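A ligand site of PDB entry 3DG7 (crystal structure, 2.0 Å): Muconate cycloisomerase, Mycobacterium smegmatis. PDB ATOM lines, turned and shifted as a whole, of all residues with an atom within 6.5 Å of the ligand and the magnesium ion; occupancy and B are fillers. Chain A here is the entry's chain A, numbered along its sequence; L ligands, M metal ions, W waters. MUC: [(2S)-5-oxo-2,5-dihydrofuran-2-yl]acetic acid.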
ATOM      1  N   LEU A  19     -12.751 -27.780  17.770  1.00  0.00           N
ATOM      2  CA  LEU A  19     -11.859 -28.098  18.877  1.00  0.00           C
ATOM      3  C   LEU A  19     -12.781 -28.503  20.025  1.00  0.00           C
ATOM      4  O   LEU A  19     -13.608 -27.713  20.476  1.00  0.00           O
ATOM      5  CB  LEU A  19     -11.014 -26.880  19.282  1.00  0.00           C
ATOM      6  CG  LEU A  19      -9.978 -27.157  20.375  1.00  0.00           C
ATOM      7  CD1 LEU A  19      -8.923 -28.114  19.843  1.00  0.00           C
ATOM      8  CD2 LEU A  19      -9.351 -25.861  20.856  1.00  0.00           C
ATOM      9  N   PHE A  21     -13.328 -30.133  23.979  1.00  0.00           N
ATOM     10  CA  PHE A  21     -12.718 -30.314  25.292  1.00  0.00           C
ATOM     11  C   PHE A  21     -13.808 -30.548  26.345  1.00  0.00           C
ATOM     12  O   PHE A  21     -14.998 -30.516  26.025  1.00  0.00           O
ATOM     13  CB  PHE A  21     -11.851 -29.085  25.637  1.00  0.00           C
ATOM     14  CG  PHE A  21     -12.467 -27.779  25.239  1.00  0.00           C
ATOM     15  CD1 PHE A  21     -13.231 -27.045  26.157  1.00  0.00           C
ATOM     16  CD2 PHE A  21     -12.319 -27.288  23.951  1.00  0.00           C
ATOM     17  CE1 PHE A  21     -13.834 -25.846  25.781  1.00  0.00           C
ATOM     18  CE2 PHE A  21     -12.920 -26.088  23.561  1.00  0.00           C
ATOM     19  CZ  PHE A  21     -13.680 -25.365  24.472  1.00  0.00           C
ATOM     20  N   SER A  23     -15.080 -28.775  28.982  1.00  0.00           N
ATOM     21  CA  SER A  23     -16.053 -27.726  29.269  1.00  0.00           C
ATOM     22  C   SER A  23     -16.882 -27.215  28.089  1.00  0.00           C
ATOM     23  O   SER A  23     -17.872 -26.506  28.294  1.00  0.00           O
ATOM     24  CB  SER A  23     -15.351 -26.549  29.955  1.00  0.00           C
ATOM     25  OG  SER A  23     -14.311 -26.027  29.148  1.00  0.00           O
ATOM     26  N   ARG A  51     -16.179 -16.774  25.570  1.00  0.00           N
ATOM     27  CA  ARG A  51     -16.099 -18.146  26.039  1.00  0.00           C
ATOM     28  C   ARG A  51     -17.084 -18.298  27.197  1.00  0.00           C
ATOM     29  O   ARG A  51     -16.710 -18.229  28.366  1.00  0.00           O
ATOM     30  CB  ARG A  51     -14.672 -18.469  26.485  1.00  0.00           C
ATOM     31  CG  ARG A  51     -13.624 -18.297  25.383  1.00  0.00           C
ATOM     32  CD  ARG A  51     -13.755 -19.362  24.305  1.00  0.00           C
ATOM     33  NE  ARG A  51     -12.826 -19.162  23.191  1.00  0.00           N
ATOM     34  CZ  ARG A  51     -13.169 -18.682  21.994  1.00  0.00           C
ATOM     35  NH1 ARG A  51     -14.423 -18.340  21.747  1.00  0.00           N
ATOM     36  NH2 ARG A  51     -12.250 -18.579  21.037  1.00  0.00           N
ATOM     37  N   PHE A  53     -18.484 -20.807  28.466  1.00  0.00           N
ATOM     38  CA  PHE A  53     -18.136 -21.933  29.321  1.00  0.00           C
ATOM     39  C   PHE A  53     -16.870 -21.693  30.138  1.00  0.00           C
ATOM     40  O   PHE A  53     -16.415 -22.580  30.860  1.00  0.00           O
ATOM     41  CB  PHE A  53     -17.975 -23.171  28.446  1.00  0.00           C
ATOM     42  CG  PHE A  53     -17.157 -22.928  27.208  1.00  0.00           C
ATOM     43  CD1 PHE A  53     -15.794 -22.635  27.298  1.00  0.00           C
ATOM     44  CD2 PHE A  53     -17.753 -22.967  25.944  1.00  0.00           C
ATOM     45  CE1 PHE A  53     -15.041 -22.389  26.142  1.00  0.00           C
ATOM     46  CE2 PHE A  53     -17.012 -22.716  24.786  1.00  0.00           C
ATOM     47  CZ  PHE A  53     -15.652 -22.424  24.890  1.00  0.00           C
ATOM     48  N   THR A  54     -16.284 -20.495  30.020  1.00  0.00           N
ATOM     49  CA  THR A  54     -15.062 -20.156  30.743  1.00  0.00           C
ATOM     50  C   THR A  54     -15.215 -18.881  31.565  1.00  0.00           C
ATOM     51  O   THR A  54     -14.854 -18.854  32.750  1.00  0.00           O
ATOM     52  CB  THR A  54     -13.856 -19.983  29.778  1.00  0.00           C
ATOM     53  OG1 THR A  54     -13.651 -21.196  29.051  1.00  0.00           O
ATOM     54  CG2 THR A  54     -12.581 -19.665  30.560  1.00  0.00           C
ATOM     55  N   TYR A  55     -15.746 -17.827  30.952  1.00  0.00           N
ATOM     56  CA  TYR A  55     -15.938 -16.547  31.637  1.00  0.00           C
ATOM     57  C   TYR A  55     -17.398 -16.095  31.636  1.00  0.00           C
ATOM     58  O   TYR A  55     -17.760 -15.164  32.348  1.00  0.00           O
ATOM     59  CB  TYR A  55     -15.098 -15.444  30.979  1.00  0.00           C
ATOM     60  CG  TYR A  55     -13.646 -15.803  30.821  1.00  0.00           C
ATOM     61  CD1 TYR A  55     -12.847 -16.063  31.938  1.00  0.00           C
ATOM     62  CD2 TYR A  55     -13.058 -15.888  29.558  1.00  0.00           C
ATOM     63  CE1 TYR A  55     -11.505 -16.402  31.798  1.00  0.00           C
ATOM     64  CE2 TYR A  55     -11.726 -16.220  29.402  1.00  0.00           C
ATOM     65  CZ  TYR A  55     -10.947 -16.485  30.529  1.00  0.00           C
ATOM     66  OH  TYR A  55      -9.629 -16.825  30.392  1.00  0.00           O
ATOM     67  N   MET A 134      -2.320 -27.593  21.579  1.00  0.00           N
ATOM     68  CA  MET A 134      -3.375 -28.235  22.360  1.00  0.00           C
ATOM     69  C   MET A 134      -4.126 -29.257  21.505  1.00  0.00           C
ATOM     70  O   MET A 134      -4.684 -28.899  20.461  1.00  0.00           O
ATOM     71  CB  MET A 134      -4.374 -27.202  22.886  1.00  0.00           C
ATOM     72  CG  MET A 134      -3.754 -26.020  23.616  1.00  0.00           C
ATOM     73  SD  MET A 134      -4.956 -24.981  24.495  1.00  0.00           S
ATOM     74  CE  MET A 134      -5.871 -24.263  23.129  1.00  0.00           C
ATOM     75  N   LYS A 160      -0.074 -30.203  24.670  1.00  0.00           N
ATOM     76  CA  LYS A 160      -0.928 -30.217  25.864  1.00  0.00           C
ATOM     77  C   LYS A 160      -2.149 -31.043  25.467  1.00  0.00           C
ATOM     78  O   LYS A 160      -2.946 -30.611  24.639  1.00  0.00           O
ATOM     79  CB  LYS A 160      -1.360 -28.808  26.279  1.00  0.00           C
ATOM     80  CG  LYS A 160      -2.263 -28.818  27.507  1.00  0.00           C
ATOM     81  CD  LYS A 160      -2.499 -27.438  28.084  1.00  0.00           C
ATOM     82  CE  LYS A 160      -3.611 -26.688  27.370  1.00  0.00           C
ATOM     83  NZ  LYS A 160      -3.891 -25.420  28.082  1.00  0.00           N
ATOM     84  N   LYS A 162      -5.775 -32.569  25.826  1.00  0.00           N
ATOM     85  CA  LYS A 162      -7.053 -32.292  26.470  1.00  0.00           C
ATOM     86  C   LYS A 162      -7.575 -33.608  27.030  1.00  0.00           C
ATOM     87  O   LYS A 162      -7.661 -34.606  26.318  1.00  0.00           O
ATOM     88  CB  LYS A 162      -8.063 -31.745  25.462  1.00  0.00           C
ATOM     89  CG  LYS A 162      -7.820 -30.321  25.004  1.00  0.00           C
ATOM     90  CD  LYS A 162      -8.020 -29.351  26.160  1.00  0.00           C
ATOM     91  CE  LYS A 162      -7.903 -27.918  25.688  1.00  0.00           C
ATOM     92  NZ  LYS A 162      -8.235 -26.984  26.787  1.00  0.00           N
ATOM     93  N   ASP A 191      -4.604 -31.079  30.328  1.00  0.00           N
ATOM     94  CA  ASP A 191      -5.575 -30.073  30.749  1.00  0.00           C
ATOM     95  C   ASP A 191      -6.945 -30.770  30.747  1.00  0.00           C
ATOM     96  O   ASP A 191      -7.437 -31.181  29.702  1.00  0.00           O
ATOM     97  CB  ASP A 191      -5.565 -28.898  29.768  1.00  0.00           C
ATOM     98  CG  ASP A 191      -6.385 -27.721  30.238  1.00  0.00           C
ATOM     99  OD1 ASP A 191      -7.306 -27.924  31.064  1.00  0.00           O
ATOM    100  OD2 ASP A 191      -6.126 -26.587  29.774  1.00  0.00           O
ATOM    101  N   ASN A 193      -9.839 -29.374  31.929  1.00  0.00           N
ATOM    102  CA  ASN A 193     -10.930 -28.409  31.878  1.00  0.00           C
ATOM    103  C   ASN A 193     -12.079 -28.716  32.850  1.00  0.00           C
ATOM    104  O   ASN A 193     -13.252 -28.660  32.478  1.00  0.00           O
ATOM    105  CB  ASN A 193     -11.476 -28.279  30.450  1.00  0.00           C
ATOM    106  CG  ASN A 193     -10.550 -27.490  29.551  1.00  0.00           C
ATOM    107  OD1 ASN A 193      -9.979 -28.019  28.593  1.00  0.00           O
ATOM    108  ND2 ASN A 193     -10.386 -26.209  29.861  1.00  0.00           N
ATOM    109  N   GLU A 217      -3.182 -29.521  34.376  1.00  0.00           N
ATOM    110  CA  GLU A 217      -3.956 -28.283  34.333  1.00  0.00           C
ATOM    111  C   GLU A 217      -5.450 -28.480  34.524  1.00  0.00           C
ATOM    112  O   GLU A 217      -6.081 -29.254  33.797  1.00  0.00           O
ATOM    113  CB  GLU A 217      -3.709 -27.562  32.989  1.00  0.00           C
ATOM    114  CG  GLU A 217      -4.371 -26.195  32.876  1.00  0.00           C
ATOM    115  CD  GLU A 217      -3.907 -25.417  31.655  1.00  0.00           C
ATOM    116  OE1 GLU A 217      -2.748 -25.647  31.224  1.00  0.00           O
ATOM    117  OE2 GLU A 217      -4.665 -24.570  31.142  1.00  0.00           O
ATOM    118  N   GLU A 218      -6.009 -27.786  35.519  1.00  0.00           N
ATOM    119  CA  GLU A 218      -7.436 -27.843  35.827  1.00  0.00           C
ATOM    120  C   GLU A 218      -8.071 -29.223  35.633  1.00  0.00           C
ATOM    121  O   GLU A 218      -9.090 -29.346  34.957  1.00  0.00           O
ATOM    122  CB  GLU A 218      -8.183 -26.815  34.964  1.00  0.00           C
ATOM    123  CG  GLU A 218      -7.793 -25.354  35.214  1.00  0.00           C
ATOM    124  CD  GLU A 218      -8.329 -24.807  36.526  1.00  0.00           C
ATOM    125  OE1 GLU A 218      -9.051 -25.550  37.221  1.00  0.00           O
ATOM    126  OE2 GLU A 218      -8.040 -23.645  36.855  1.00  0.00           O
ATOM    127  N   ILE A 240      -1.406 -26.390  37.206  1.00  0.00           N
ATOM    128  CA  ILE A 240      -1.767 -25.122  36.599  1.00  0.00           C
ATOM    129  C   ILE A 240      -3.234 -24.724  36.757  1.00  0.00           C
ATOM    130  O   ILE A 240      -4.127 -25.481  36.389  1.00  0.00           O
ATOM    131  CB  ILE A 240      -1.468 -25.115  35.082  1.00  0.00           C
ATOM    132  CG1 ILE A 240       0.028 -25.347  34.834  1.00  0.00           C
ATOM    133  CG2 ILE A 240      -1.909 -23.780  34.465  1.00  0.00           C
ATOM    134  CD1 ILE A 240       0.404 -25.454  33.357  1.00  0.00           C
ATOM    135  N   ASP A 242      -6.116 -22.211  35.584  1.00  0.00           N
ATOM    136  CA  ASP A 242      -6.396 -21.468  34.356  1.00  0.00           C
ATOM    137  C   ASP A 242      -7.701 -20.698  34.502  1.00  0.00           C
ATOM    138  O   ASP A 242      -7.703 -19.531  34.924  1.00  0.00           O
ATOM    139  CB  ASP A 242      -6.464 -22.456  33.179  1.00  0.00           C
ATOM    140  CG  ASP A 242      -6.837 -21.800  31.848  1.00  0.00           C
ATOM    141  OD1 ASP A 242      -7.043 -20.576  31.805  1.00  0.00           O
ATOM    142  OD2 ASP A 242      -6.930 -22.533  30.847  1.00  0.00           O
ATOM    143  N   GLU A 243      -8.822 -21.337  34.182  1.00  0.00           N
ATOM    144  CA  GLU A 243     -10.106 -20.657  34.289  1.00  0.00           C
ATOM    145  C   GLU A 243     -10.449 -20.218  35.721  1.00  0.00           C
ATOM    146  O   GLU A 243     -11.278 -19.333  35.919  1.00  0.00           O
ATOM    147  CB  GLU A 243     -11.231 -21.530  33.733  1.00  0.00           C
ATOM    148  CG  GLU A 243     -11.274 -22.957  34.247  1.00  0.00           C
ATOM    149  CD  GLU A 243     -10.647 -23.941  33.262  1.00  0.00           C
ATOM    150  OE1 GLU A 243     -11.308 -24.954  32.950  1.00  0.00           O
ATOM    151  OE2 GLU A 243      -9.505 -23.692  32.817  1.00  0.00           O
ATOM    152  N   SER A 264      -1.519 -20.092  34.836  1.00  0.00           N
ATOM    153  CA  SER A 264      -1.668 -19.906  33.412  1.00  0.00           C
ATOM    154  C   SER A 264      -1.903 -18.419  33.170  1.00  0.00           C
ATOM    155  O   SER A 264      -2.708 -17.785  33.856  1.00  0.00           O
ATOM    156  CB  SER A 264      -2.875 -20.699  32.905  1.00  0.00           C
ATOM    157  OG  SER A 264      -3.333 -20.196  31.654  1.00  0.00           O
ATOM    158  N   LYS A 266      -3.087 -15.803  30.270  1.00  0.00           N
ATOM    159  CA  LYS A 266      -3.682 -15.701  28.939  1.00  0.00           C
ATOM    160  C   LYS A 266      -3.980 -14.248  28.661  1.00  0.00           C
ATOM    161  O   LYS A 266      -4.771 -13.612  29.365  1.00  0.00           O
ATOM    162  CB  LYS A 266      -4.970 -16.539  28.861  1.00  0.00           C
ATOM    163  CG  LYS A 266      -4.720 -18.048  28.931  1.00  0.00           C
ATOM    164  CD  LYS A 266      -5.996 -18.843  28.685  1.00  0.00           C
ATOM    165  CE  LYS A 266      -5.757 -20.331  28.784  1.00  0.00           C
ATOM    166  NZ  LYS A 266      -6.970 -21.104  28.379  1.00  0.00           N
ATOM    167  N   GLY A 292      -0.922 -19.414  28.130  1.00  0.00           N
ATOM    168  CA  GLY A 292      -1.951 -20.300  27.619  1.00  0.00           C
ATOM    169  C   GLY A 292      -2.647 -19.790  26.376  1.00  0.00           C
ATOM    170  O   GLY A 292      -2.417 -18.659  25.942  1.00  0.00           O
ATOM    171  N   ASN A 293      -3.508 -20.627  25.812  1.00  0.00           N
ATOM    172  CA  ASN A 293      -4.251 -20.308  24.595  1.00  0.00           C
ATOM    173  C   ASN A 293      -5.746 -20.297  24.925  1.00  0.00           C
ATOM    174  O   ASN A 293      -6.252 -21.234  25.534  1.00  0.00           O
ATOM    175  CB  ASN A 293      -3.944 -21.345  23.518  1.00  0.00           C
ATOM    176  CG  ASN A 293      -4.436 -20.928  22.138  1.00  0.00           C
ATOM    177  OD1 ASN A 293      -5.636 -20.880  21.883  1.00  0.00           O
ATOM    178  ND2 ASN A 293      -3.496 -20.634  21.236  1.00  0.00           N
ATOM    179  N   GLN A 294      -6.434 -19.234  24.522  1.00  0.00           N
ATOM    180  CA  GLN A 294      -7.872 -19.101  24.765  1.00  0.00           C
ATOM    181  C   GLN A 294      -8.621 -19.536  23.498  1.00  0.00           C
ATOM    182  O   GLN A 294      -9.756 -19.113  23.257  1.00  0.00           O
ATOM    183  CB  GLN A 294      -8.181 -17.626  25.063  1.00  0.00           C
ATOM    184  CG  GLN A 294      -9.488 -17.384  25.800  1.00  0.00           C
ATOM    185  CD  GLN A 294      -9.351 -17.631  27.296  1.00  0.00           C
ATOM    186  OE1 GLN A 294      -8.816 -16.807  28.031  1.00  0.00           O
ATOM    187  NE2 GLN A 294      -9.831 -18.781  27.734  1.00  0.00           N
ATOM    188  N   ILE A 295      -7.986 -20.414  22.717  1.00  0.00           N
ATOM    189  CA  ILE A 295      -8.509 -20.872  21.431  1.00  0.00           C
ATOM    190  C   ILE A 295      -8.534 -19.598  20.603  1.00  0.00           C
ATOM    191  O   ILE A 295      -9.532 -19.244  19.963  1.00  0.00           O
ATOM    192  CB  ILE A 295      -9.931 -21.468  21.544  1.00  0.00           C
ATOM    193  CG1 ILE A 295      -9.974 -22.539  22.643  1.00  0.00           C
ATOM    194  CG2 ILE A 295     -10.298 -22.136  20.218  1.00  0.00           C
ATOM    195  CD1 ILE A 295     -11.357 -23.107  22.895  1.00  0.00           C
ATOM    196  N   GLU A 320       1.419 -21.697  24.367  1.00  0.00           N
ATOM    197  CA  GLU A 320       0.347 -22.305  23.582  1.00  0.00           C
ATOM    198  C   GLU A 320      -0.032 -21.293  22.496  1.00  0.00           C
ATOM    199  O   GLU A 320      -0.890 -20.427  22.681  1.00  0.00           O
ATOM    200  CB  GLU A 320      -0.821 -22.631  24.520  1.00  0.00           C
ATOM    201  CG  GLU A 320      -0.488 -23.841  25.387  1.00  0.00           C
ATOM    202  CD  GLU A 320      -1.276 -23.900  26.697  1.00  0.00           C
ATOM    203  OE1 GLU A 320      -2.454 -23.490  26.721  1.00  0.00           O
ATOM    204  OE2 GLU A 320      -0.695 -24.381  27.698  1.00  0.00           O
HETATM  205  C1  MUC L   1      -7.391 -24.152  28.034  1.00  0.00           C
HETATM  206  O1  MUC L   1      -6.178 -23.994  28.330  1.00  0.00           O
HETATM  207  O2  MUC L   1      -8.315 -24.384  28.850  1.00  0.00           O
HETATM  208  C4  MUC L   1     -10.359 -24.359  26.625  1.00  0.00           C
HETATM  209  C5  MUC L   1     -11.316 -23.451  26.867  1.00  0.00           C
HETATM  210  C6  MUC L   1     -10.769 -22.227  26.823  1.00  0.00           C
HETATM  211  O6  MUC L   1     -11.405 -21.174  26.840  1.00  0.00           O
HETATM  212  O3  MUC L   1      -9.403 -22.270  26.755  1.00  0.00           O
HETATM  213  C3  MUC L   1      -9.153 -23.533  26.154  1.00  0.00           C
HETATM  214  C2  MUC L   1      -7.742 -24.087  26.513  1.00  0.00           C
HETATM  215 MG    MG M   1      -6.483 -24.632  30.269  1.00  0.00          MG
HETATM  216  O   HOH W   1      -7.749 -25.255  31.755  1.00  0.00           O
HETATM  217  O   HOH W   2     -10.338 -22.985  29.980  1.00  0.00           O
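The magnesium ion is bound by the side-chain carboxylate (OE2) of Glu 217, the side-chain carboxylate (OD2) of Asp 191, water W1, an oxygen (O1) of the ligand, the side-chain carboxylate (OD2) of Asp 242 and an oxygen (O2) of the ligand.
Water W1 lies within hydrogen-bond range of the side-chain carboxylate (OE2) of Glu 243 (2.6 Å), the side-chain carboxylate (OD1) of Asp 191 (2.8 Å) and the side-chain amide nitrogen (ND2) of Asn 193 (3.4 Å).
Water W2 lies within hydrogen-bond range of OE2 of Glu 243 (3.0 Å), ND2 of Asn 193 (3.2 Å) and O3 of the ligand (3.4 Å).
NZ of Lys 160 touches the magnesium ion, at 3.5 Å.
Of the 24 residues printed, 4 come within 4 Å of the magnesium ion.
The nearest printed residue that does not touch the magnesium ion is Lys 266 (4.03 Å).
The side-chain amino group (NZ) of Lys 160 sits close to an oxygen (O1) of the ligand.
ND2 of Asn 193 sits close to O2 of the ligand (2.9 Å).
An oxygen (O3) of the ligand lies close to the side-chain amino group (NZ) of Lys 266.
O2 of the ligand lies close to NZ of Lys 162, at 3.3 Å.
NE2 of Gln 294 sits at hydrogen-bond distance from O6 of the ligand (3.0 Å).
An oxygen (O6) of the ligand lies within hydrogen-bond range of the side-chain hydroxyl of Thr 54, at 3.2 Å.
NZ of Lys 160 lies close to SD of Met 134.
The backbone NH of Ile 295 lies within hydrogen-bond range of the side-chain amide oxygen of Asn 293 (2.5 Å).
The backbone NH (N) of Asn 193 is in hydrogen-bond range of the backbone carbonyl oxygen (O) of Glu 218 (3.1 Å).
The side-chain amide oxygen (OE1) of Gln 294 sits at hydrogen-bond distance from the side-chain hydroxyl (OH) of Tyr 55.
OD2 of Asp 191 lies close to NZ of Lys 162.
OE1 of Glu 243 is in hydrogen-bond range of ND2 of Asn 193 (3.5 Å).
N of Asp 242 lies within hydrogen-bond range of OE2 of Glu 218 (2.7 Å).
OD1 of Asp 242 is in salt-bridge range of NZ of Lys 266 (3.5 Å).
Residues that only touch the ligand: Asn 293, Met 134, Phe 21, Ile 295, Phe 53 and Arg 51.
15 residues have an atom within 4 Å of the ligand: Phe 21, Arg 51, Phe 53, Thr 54, Met 134, Lys 160, Lys 162, Asp 191, Asn 193, Glu 217, Asp 242, Lys 266, Asn 293, Gln 294 and Ile 295.
The nearest printed residue that does not touch the ligand is Glu 320 (4.1 Å).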
